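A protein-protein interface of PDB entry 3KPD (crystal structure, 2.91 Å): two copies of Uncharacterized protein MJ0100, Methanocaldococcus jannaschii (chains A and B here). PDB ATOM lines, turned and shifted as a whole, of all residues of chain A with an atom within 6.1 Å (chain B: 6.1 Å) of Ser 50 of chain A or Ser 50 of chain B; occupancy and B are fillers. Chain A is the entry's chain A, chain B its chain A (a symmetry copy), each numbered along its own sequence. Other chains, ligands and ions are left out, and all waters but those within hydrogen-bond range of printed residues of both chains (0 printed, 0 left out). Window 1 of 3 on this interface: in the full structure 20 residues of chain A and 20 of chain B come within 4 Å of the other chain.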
ATOM      1  N   LEU A  27      16.054  -5.774  32.262  1.00  0.00           N
ATOM      2  CA  LEU A  27      17.362  -5.380  32.808  1.00  0.00           C
ATOM      3  C   LEU A  27      17.414  -3.902  33.186  1.00  0.00           C
ATOM      4  O   LEU A  27      17.764  -3.551  34.306  1.00  0.00           O
ATOM      5  CB  LEU A  27      18.486  -5.672  31.808  1.00  0.00           C
ATOM      6  CG  LEU A  27      18.825  -7.074  31.301  1.00  0.00           C
ATOM      7  CD1 LEU A  27      20.055  -6.995  30.445  1.00  0.00           C
ATOM      8  CD2 LEU A  27      19.058  -8.073  32.420  1.00  0.00           C
ATOM      9  N   ASN A  33      21.987  -6.635  35.663  1.00  0.00           N
ATOM     10  CA  ASN A  33      22.694  -7.119  34.487  1.00  0.00           C
ATOM     11  C   ASN A  33      22.557  -8.618  34.241  1.00  0.00           C
ATOM     12  O   ASN A  33      23.219  -9.154  33.364  1.00  0.00           O
ATOM     13  CB  ASN A  33      24.165  -6.721  34.513  1.00  0.00           C
ATOM     14  CG  ASN A  33      24.838  -6.901  33.162  1.00  0.00           C
ATOM     15  OD1 ASN A  33      24.218  -6.716  32.121  1.00  0.00           O
ATOM     16  ND2 ASN A  33      26.104  -7.269  33.176  1.00  0.00           N
ATOM     17  N   HIS A  34      21.688  -9.289  34.992  1.00  0.00           N
ATOM     18  CA  HIS A  34      21.612 -10.745  34.932  1.00  0.00           C
ATOM     19  C   HIS A  34      20.190 -11.177  34.927  1.00  0.00           C
ATOM     20  O   HIS A  34      19.436 -10.847  35.837  1.00  0.00           O
ATOM     21  CB  HIS A  34      22.329 -11.381  36.125  1.00  0.00           C
ATOM     22  CG  HIS A  34      23.805 -11.164  36.112  1.00  0.00           C
ATOM     23  ND1 HIS A  34      24.400 -10.061  36.680  1.00  0.00           N
ATOM     24  CD2 HIS A  34      24.804 -11.884  35.548  1.00  0.00           C
ATOM     25  CE1 HIS A  34      25.706 -10.128  36.494  1.00  0.00           C
ATOM     26  NE2 HIS A  34      25.977 -11.222  35.807  1.00  0.00           N
ATOM     27  N   ILE A  48      20.706 -14.741  30.547  1.00  0.00           N
ATOM     28  CA  ILE A  48      20.942 -13.588  29.687  1.00  0.00           C
ATOM     29  C   ILE A  48      21.538 -12.443  30.496  1.00  0.00           C
ATOM     30  O   ILE A  48      21.142 -12.213  31.632  1.00  0.00           O
ATOM     31  CB  ILE A  48      19.648 -13.142  28.968  1.00  0.00           C
ATOM     32  CG1 ILE A  48      19.249 -14.174  27.915  1.00  0.00           C
ATOM     33  CG2 ILE A  48      19.823 -11.786  28.294  1.00  0.00           C
ATOM     34  CD1 ILE A  48      20.220 -14.259  26.768  1.00  0.00           C
ATOM     35  N   THR A  49      22.520 -11.765  29.914  1.00  0.00           N
ATOM     36  CA  THR A  49      23.065 -10.536  30.470  1.00  0.00           C
ATOM     37  C   THR A  49      23.187  -9.561  29.313  1.00  0.00           C
ATOM     38  O   THR A  49      23.155  -9.982  28.163  1.00  0.00           O
ATOM     39  CB  THR A  49      24.462 -10.733  31.087  1.00  0.00           C
ATOM     40  OG1 THR A  49      25.442 -10.846  30.045  1.00  0.00           O
ATOM     41  CG2 THR A  49      24.517 -11.964  31.984  1.00  0.00           C
ATOM     42  N   SER A  50      23.352  -8.273  29.601  1.00  0.00           N
ATOM     43  CA  SER A  50      23.427  -7.241  28.558  1.00  0.00           C
ATOM     44  C   SER A  50      24.402  -7.558  27.425  1.00  0.00           C
ATOM     45  O   SER A  50      24.291  -7.014  26.323  1.00  0.00           O
ATOM     46  CB  SER A  50      23.818  -5.906  29.171  1.00  0.00           C
ATOM     47  OG  SER A  50      25.147  -5.974  29.643  1.00  0.00           O
ATOM     48  N   TRP A  51      25.371  -8.420  27.712  1.00  0.00           N
ATOM     49  CA  TRP A  51      26.316  -8.862  26.706  1.00  0.00           C
ATOM     50  C   TRP A  51      25.604  -9.608  25.581  1.00  0.00           C
ATOM     51  O   TRP A  51      25.858  -9.357  24.401  1.00  0.00           O
ATOM     52  CB  TRP A  51      27.363  -9.760  27.334  1.00  0.00           C
ATOM     53  CG  TRP A  51      28.224 -10.408  26.309  1.00  0.00           C
ATOM     54  CD1 TRP A  51      28.045 -11.642  25.727  1.00  0.00           C
ATOM     55  CD2 TRP A  51      29.389  -9.848  25.705  1.00  0.00           C
ATOM     56  NE1 TRP A  51      29.041 -11.876  24.811  1.00  0.00           N
ATOM     57  CE2 TRP A  51      29.883 -10.794  24.789  1.00  0.00           C
ATOM     58  CE3 TRP A  51      30.075  -8.644  25.869  1.00  0.00           C
ATOM     59  CZ2 TRP A  51      31.023 -10.577  24.053  1.00  0.00           C
ATOM     60  CZ3 TRP A  51      31.195  -8.428  25.129  1.00  0.00           C
ATOM     61  CH2 TRP A  51      31.660  -9.385  24.230  1.00  0.00           C
ATOM     62  N   ASP A  52      24.727 -10.535  25.954  1.00  0.00           N
ATOM     63  CA  ASP A  52      23.898 -11.237  24.989  1.00  0.00           C
ATOM     64  C   ASP A  52      23.032 -10.262  24.175  1.00  0.00           C
ATOM     65  O   ASP A  52      22.876 -10.432  22.971  1.00  0.00           O
ATOM     66  CB  ASP A  52      23.022 -12.277  25.687  1.00  0.00           C
ATOM     67  CG  ASP A  52      23.811 -13.174  26.636  1.00  0.00           C
ATOM     68  OD1 ASP A  52      24.756 -13.857  26.193  1.00  0.00           O
ATOM     69  OD2 ASP A  52      23.482 -13.208  27.839  1.00  0.00           O
ATOM     70  N   ILE A  53      22.483  -9.230  24.806  1.00  0.00           N
ATOM     71  CA  ILE A  53      21.669  -8.274  24.054  1.00  0.00           C
ATOM     72  C   ILE A  53      22.515  -7.663  22.936  1.00  0.00           C
ATOM     73  O   ILE A  53      22.032  -7.442  21.827  1.00  0.00           O
ATOM     74  CB  ILE A  53      21.050  -7.138  24.933  1.00  0.00           C
ATOM     75  CG1 ILE A  53      20.582  -7.634  26.320  1.00  0.00           C
ATOM     76  CG2 ILE A  53      19.907  -6.469  24.207  1.00  0.00           C
ATOM     77  CD1 ILE A  53      19.337  -8.522  26.337  1.00  0.00           C
ATOM     78  N   ALA A  54      23.783  -7.401  23.222  1.00  0.00           N
ATOM     79  CA  ALA A  54      24.656  -6.796  22.227  1.00  0.00           C
ATOM     80  C   ALA A  54      25.170  -7.848  21.228  1.00  0.00           C
ATOM     81  O   ALA A  54      25.527  -7.525  20.090  1.00  0.00           O
ATOM     82  CB  ALA A  54      25.786  -6.062  22.890  1.00  0.00           C
ATOM     83  N   LYS A  55      25.201  -9.108  21.648  1.00  0.00           N
ATOM     84  CA  LYS A  55      25.464 -10.192  20.717  1.00  0.00           C
ATOM     85  C   LYS A  55      24.290 -10.256  19.709  1.00  0.00           C
ATOM     86  O   LYS A  55      24.509 -10.373  18.500  1.00  0.00           O
ATOM     87  CB  LYS A  55      25.651 -11.515  21.475  1.00  0.00           C
ATOM     88  CG  LYS A  55      26.145 -12.692  20.647  1.00  0.00           C
ATOM     89  CD  LYS A  55      27.674 -12.890  20.690  1.00  0.00           C
ATOM     90  CE  LYS A  55      28.114 -13.892  21.783  1.00  0.00           C
ATOM     91  NZ  LYS A  55      29.511 -14.430  21.606  1.00  0.00           N
ATOM     92  N   LEU B  27      32.681  -4.533  20.129  1.00  0.00           N
ATOM     93  CA  LEU B  27      32.711  -5.309  21.378  1.00  0.00           C
ATOM     94  C   LEU B  27      32.753  -6.815  21.127  1.00  0.00           C
ATOM     95  O   LEU B  27      33.619  -7.513  21.638  1.00  0.00           O
ATOM     96  CB  LEU B  27      31.495  -4.992  22.254  1.00  0.00           C
ATOM     97  CG  LEU B  27      31.197  -3.601  22.817  1.00  0.00           C
ATOM     98  CD1 LEU B  27      30.008  -3.692  23.728  1.00  0.00           C
ATOM     99  CD2 LEU B  27      32.367  -3.004  23.578  1.00  0.00           C
ATOM    100  N   ASN B  33      34.205  -5.807  26.729  1.00  0.00           N
ATOM    101  CA  ASN B  33      32.990  -5.177  27.225  1.00  0.00           C
ATOM    102  C   ASN B  33      33.101  -3.671  27.435  1.00  0.00           C
ATOM    103  O   ASN B  33      32.188  -3.063  27.976  1.00  0.00           O
ATOM    104  CB  ASN B  33      32.485  -5.852  28.495  1.00  0.00           C
ATOM    105  CG  ASN B  33      31.058  -5.456  28.832  1.00  0.00           C
ATOM    106  OD1 ASN B  33      30.241  -5.230  27.947  1.00  0.00           O
ATOM    107  ND2 ASN B  33      30.757  -5.365  30.113  1.00  0.00           N
ATOM    108  N   HIS B  34      34.200  -3.066  26.991  1.00  0.00           N
ATOM    109  CA  HIS B  34      34.456  -1.662  27.294  1.00  0.00           C
ATOM    110  C   HIS B  34      34.972  -0.970  26.084  1.00  0.00           C
ATOM    111  O   HIS B  34      35.984  -1.373  25.520  1.00  0.00           O
ATOM    112  CB  HIS B  34      35.474  -1.522  28.428  1.00  0.00           C
ATOM    113  CG  HIS B  34      34.967  -2.016  29.742  1.00  0.00           C
ATOM    114  ND1 HIS B  34      35.095  -3.327  30.142  1.00  0.00           N
ATOM    115  CD2 HIS B  34      34.280  -1.385  30.723  1.00  0.00           C
ATOM    116  CE1 HIS B  34      34.536  -3.474  31.330  1.00  0.00           C
ATOM    117  NE2 HIS B  34      34.031  -2.312  31.703  1.00  0.00           N
ATOM    118  N   ILE B  48      31.444   3.457  26.425  1.00  0.00           N
ATOM    119  CA  ILE B  48      30.342   2.551  26.123  1.00  0.00           C
ATOM    120  C   ILE B  48      30.685   1.137  26.574  1.00  0.00           C
ATOM    121  O   ILE B  48      31.819   0.697  26.427  1.00  0.00           O
ATOM    122  CB  ILE B  48      29.980   2.579  24.620  1.00  0.00           C
ATOM    123  CG1 ILE B  48      29.326   3.913  24.262  1.00  0.00           C
ATOM    124  CG2 ILE B  48      29.029   1.445  24.254  1.00  0.00           C
ATOM    125  CD1 ILE B  48      27.978   4.107  24.904  1.00  0.00           C
ATOM    126  N   THR B  49      29.709   0.457  27.163  1.00  0.00           N
ATOM    127  CA  THR B  49      29.816  -0.959  27.481  1.00  0.00           C
ATOM    128  C   THR B  49      28.507  -1.593  27.047  1.00  0.00           C
ATOM    129  O   THR B  49      27.530  -0.883  26.844  1.00  0.00           O
ATOM    130  CB  THR B  49      30.002  -1.213  28.989  1.00  0.00           C
ATOM    131  OG1 THR B  49      28.755  -1.024  29.672  1.00  0.00           O
ATOM    132  CG2 THR B  49      31.065  -0.302  29.591  1.00  0.00           C
ATOM    133  N   SER B  50      28.469  -2.917  26.930  1.00  0.00           N
ATOM    134  CA  SER B  50      27.270  -3.628  26.465  1.00  0.00           C
ATOM    135  C   SER B  50      25.980  -3.221  27.174  1.00  0.00           C
ATOM    136  O   SER B  50      24.879  -3.417  26.653  1.00  0.00           O
ATOM    137  CB  SER B  50      27.455  -5.128  26.625  1.00  0.00           C
ATOM    138  OG  SER B  50      27.502  -5.453  27.999  1.00  0.00           O
ATOM    139  N   TRP B  51      26.122  -2.676  28.378  1.00  0.00           N
ATOM    140  CA  TRP B  51      24.984  -2.179  29.126  1.00  0.00           C
ATOM    141  C   TRP B  51      24.303  -1.034  28.381  1.00  0.00           C
ATOM    142  O   TRP B  51      23.076  -1.007  28.258  1.00  0.00           O
ATOM    143  CB  TRP B  51      25.428  -1.708  30.496  1.00  0.00           C
ATOM    144  CG  TRP B  51      24.338  -0.994  31.216  1.00  0.00           C
ATOM    145  CD1 TRP B  51      24.097   0.360  31.234  1.00  0.00           C
ATOM    146  CD2 TRP B  51      23.309  -1.593  32.001  1.00  0.00           C
ATOM    147  NE1 TRP B  51      22.986   0.626  31.995  1.00  0.00           N
ATOM    148  CE2 TRP B  51      22.493  -0.555  32.485  1.00  0.00           C
ATOM    149  CE3 TRP B  51      23.013  -2.910  32.359  1.00  0.00           C
ATOM    150  CZ2 TRP B  51      21.416  -0.791  33.306  1.00  0.00           C
ATOM    151  CZ3 TRP B  51      21.939  -3.139  33.160  1.00  0.00           C
ATOM    152  CH2 TRP B  51      21.149  -2.089  33.625  1.00  0.00           C
ATOM    153  N   ASP B  52      25.102  -0.084  27.905  1.00  0.00           N
ATOM    154  CA  ASP B  52      24.597   0.998  27.080  1.00  0.00           C
ATOM    155  C   ASP B  52      23.909   0.469  25.812  1.00  0.00           C
ATOM    156  O   ASP B  52      22.870   0.981  25.412  1.00  0.00           O
ATOM    157  CB  ASP B  52      25.721   1.968  26.716  1.00  0.00           C
ATOM    158  CG  ASP B  52      26.541   2.404  27.926  1.00  0.00           C
ATOM    159  OD1 ASP B  52      25.977   2.978  28.877  1.00  0.00           O
ATOM    160  OD2 ASP B  52      27.769   2.181  27.927  1.00  0.00           O
ATOM    161  N   ILE B  53      24.459  -0.563  25.183  1.00  0.00           N
ATOM    162  CA  ILE B  53      23.818  -1.104  23.982  1.00  0.00           C
ATOM    163  C   ILE B  53      22.397  -1.549  24.329  1.00  0.00           C
ATOM    164  O   ILE B  53      21.468  -1.366  23.545  1.00  0.00           O
ATOM    165  CB  ILE B  53      24.600  -2.286  23.321  1.00  0.00           C
ATOM    166  CG1 ILE B  53      26.133  -2.095  23.363  1.00  0.00           C
ATOM    167  CG2 ILE B  53      24.140  -2.496  21.899  1.00  0.00           C
ATOM    168  CD1 ILE B  53      26.706  -1.014  22.445  1.00  0.00           C
ATOM    169  N   ALA B  54      22.224  -2.124  25.511  1.00  0.00           N
ATOM    170  CA  ALA B  54      20.910  -2.604  25.915  1.00  0.00           C
ATOM    171  C   ALA B  54      20.033  -1.448  26.425  1.00  0.00           C
ATOM    172  O   ALA B  54      18.799  -1.519  26.388  1.00  0.00           O
ATOM    173  CB  ALA B  54      21.036  -3.697  26.937  1.00  0.00           C
ATOM    174  N   LYS B  55      20.664  -0.378  26.894  1.00  0.00           N
ATOM    175  CA  LYS B  55      19.932   0.841  27.197  1.00  0.00           C
ATOM    176  C   LYS B  55      19.365   1.403  25.870  1.00  0.00           C
ATOM    177  O   LYS B  55      18.196   1.793  25.805  1.00  0.00           O
ATOM    178  CB  LYS B  55      20.844   1.850  27.913  1.00  0.00           C
ATOM    179  CG  LYS B  55      20.155   3.083  28.481  1.00  0.00           C
ATOM    180  CD  LYS B  55      19.768   2.952  29.968  1.00  0.00           C
ATOM    181  CE  LYS B  55      20.850   3.520  30.916  1.00  0.00           C
ATOM    182  NZ  LYS B  55      20.366   3.796  32.317  1.00  0.00           N
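The side-chain hydroxyl (OG) of Ser 50 of chain B lies within hydrogen-bond range of the side-chain hydroxyl (OG) of Ser 50 of chain A, at 2.9 Å.
OG1 of Thr 49 of chain B lies close to N of Trp 51 of chain B (3.4 Å). OD1 of Asn 33 of chain A sits at hydrogen-bond distance from OG of Ser 50 of chain A (2.7 Å). The side-chain hydroxyl (OG1) of Thr 49 of chain A lies close to the backbone NH (N) of Trp 51 of chain A (3.4 Å). OD1 of Asn 33 of chain B sits at hydrogen-bond distance from OG of Ser 50 of chain B (2.7 Å).
Trp 51 of chain B touches Leu 27 of chain A (CH2 to O, 3.7 Å). OD1 of Asn 33 of chain A touches CE3 of Trp 51 of chain B, at 3.999 Å. Ser 50 of chain A touches Trp 51 of chain B. CH2 of Trp 51 of chain A touches O of Leu 27 of chain B (3.7 Å). OG of Ser 50 of chain B touches N of Trp 51 of chain A (3.7 Å). Ile 53 of chain A touches Ala 54 of chain B. Ile 53 of chain B touches Ala 54 of chain A.
Of the printed residues of chain B, Asn 33 of chain A touches Trp 51. Of chain B, only Ser 50 and Trp 51 come within 4 Å of Ser 50 of chain A. Of the printed residues of chain B, Trp 51 of chain A touches Leu 27 (3.7 Å) and Ser 50 (3.7 Å). Of the printed residues of chain A, Leu 27 of chain B touches Trp 51. Of chain A, only Ser 50 and Trp 51 come within 4 Å of Ser 50 of chain B. Of the printed residues of chain A, Ile 53 of chain B touches Ala 54 (3.98 Å). Printed residues of chain A within 4 Å of Ala 54 of chain B: Ile 53. The nearest residue of chain B that does not touch Ser 50 of chain A is Ala 54 of chain B (4.2 Å). The nearest residue of chain A that does not touch Ser 50 of chain B is Ala 54 of chain A (4.2 Å). The nearest printed residue of chain B that does not touch Trp 51 of chain A is Asn 33 of chain B (4.0001 Å).
Of the 11 printed residues of chain B, 5 touch a printed residue of chain A. Printed residues of chain B that touch a printed residue of chain A: Leu 27, Ser 50, Trp 51, Ile 53 and Ala 54. Hydrophobic or aromatic side chains of chain B that line the printed part of chain A: Trp 51, Ile 53 and Ala 54. Of the 11 printed residues of chain A, 6 touch a printed residue of chain B. Hydrophobic or aromatic side chains of chain A within 4 Å of the printed part of chain B: Trp 51, Ile 53 and Ala 54.
Leu 27 of chain A touches Trp 51 of chain B, and with the chains exchanged Trp 51 of chain A touches Leu 27 of chain B. Asn 33 of chain A touches Trp 51 of chain B, but with the chains exchanged Trp 51 of chain A does not touch Asn 33 of chain B (4.0001 Å). Ser 50 of chain A touches its own counterpart, Ser 50 of chain B. Ile 53 of chain A touches Ala 54 of chain B, and with the chains exchanged Ala 54 of chain A touches Ile 53 of chain B. Positions printed for both chains: 27, 33, 34, 48, 49, 50, 51, 52, 53, 54 and 55. Of the 8 pairs that touch across the chains among the printed residues, 7 have their exchanged pair printed and touching as well.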
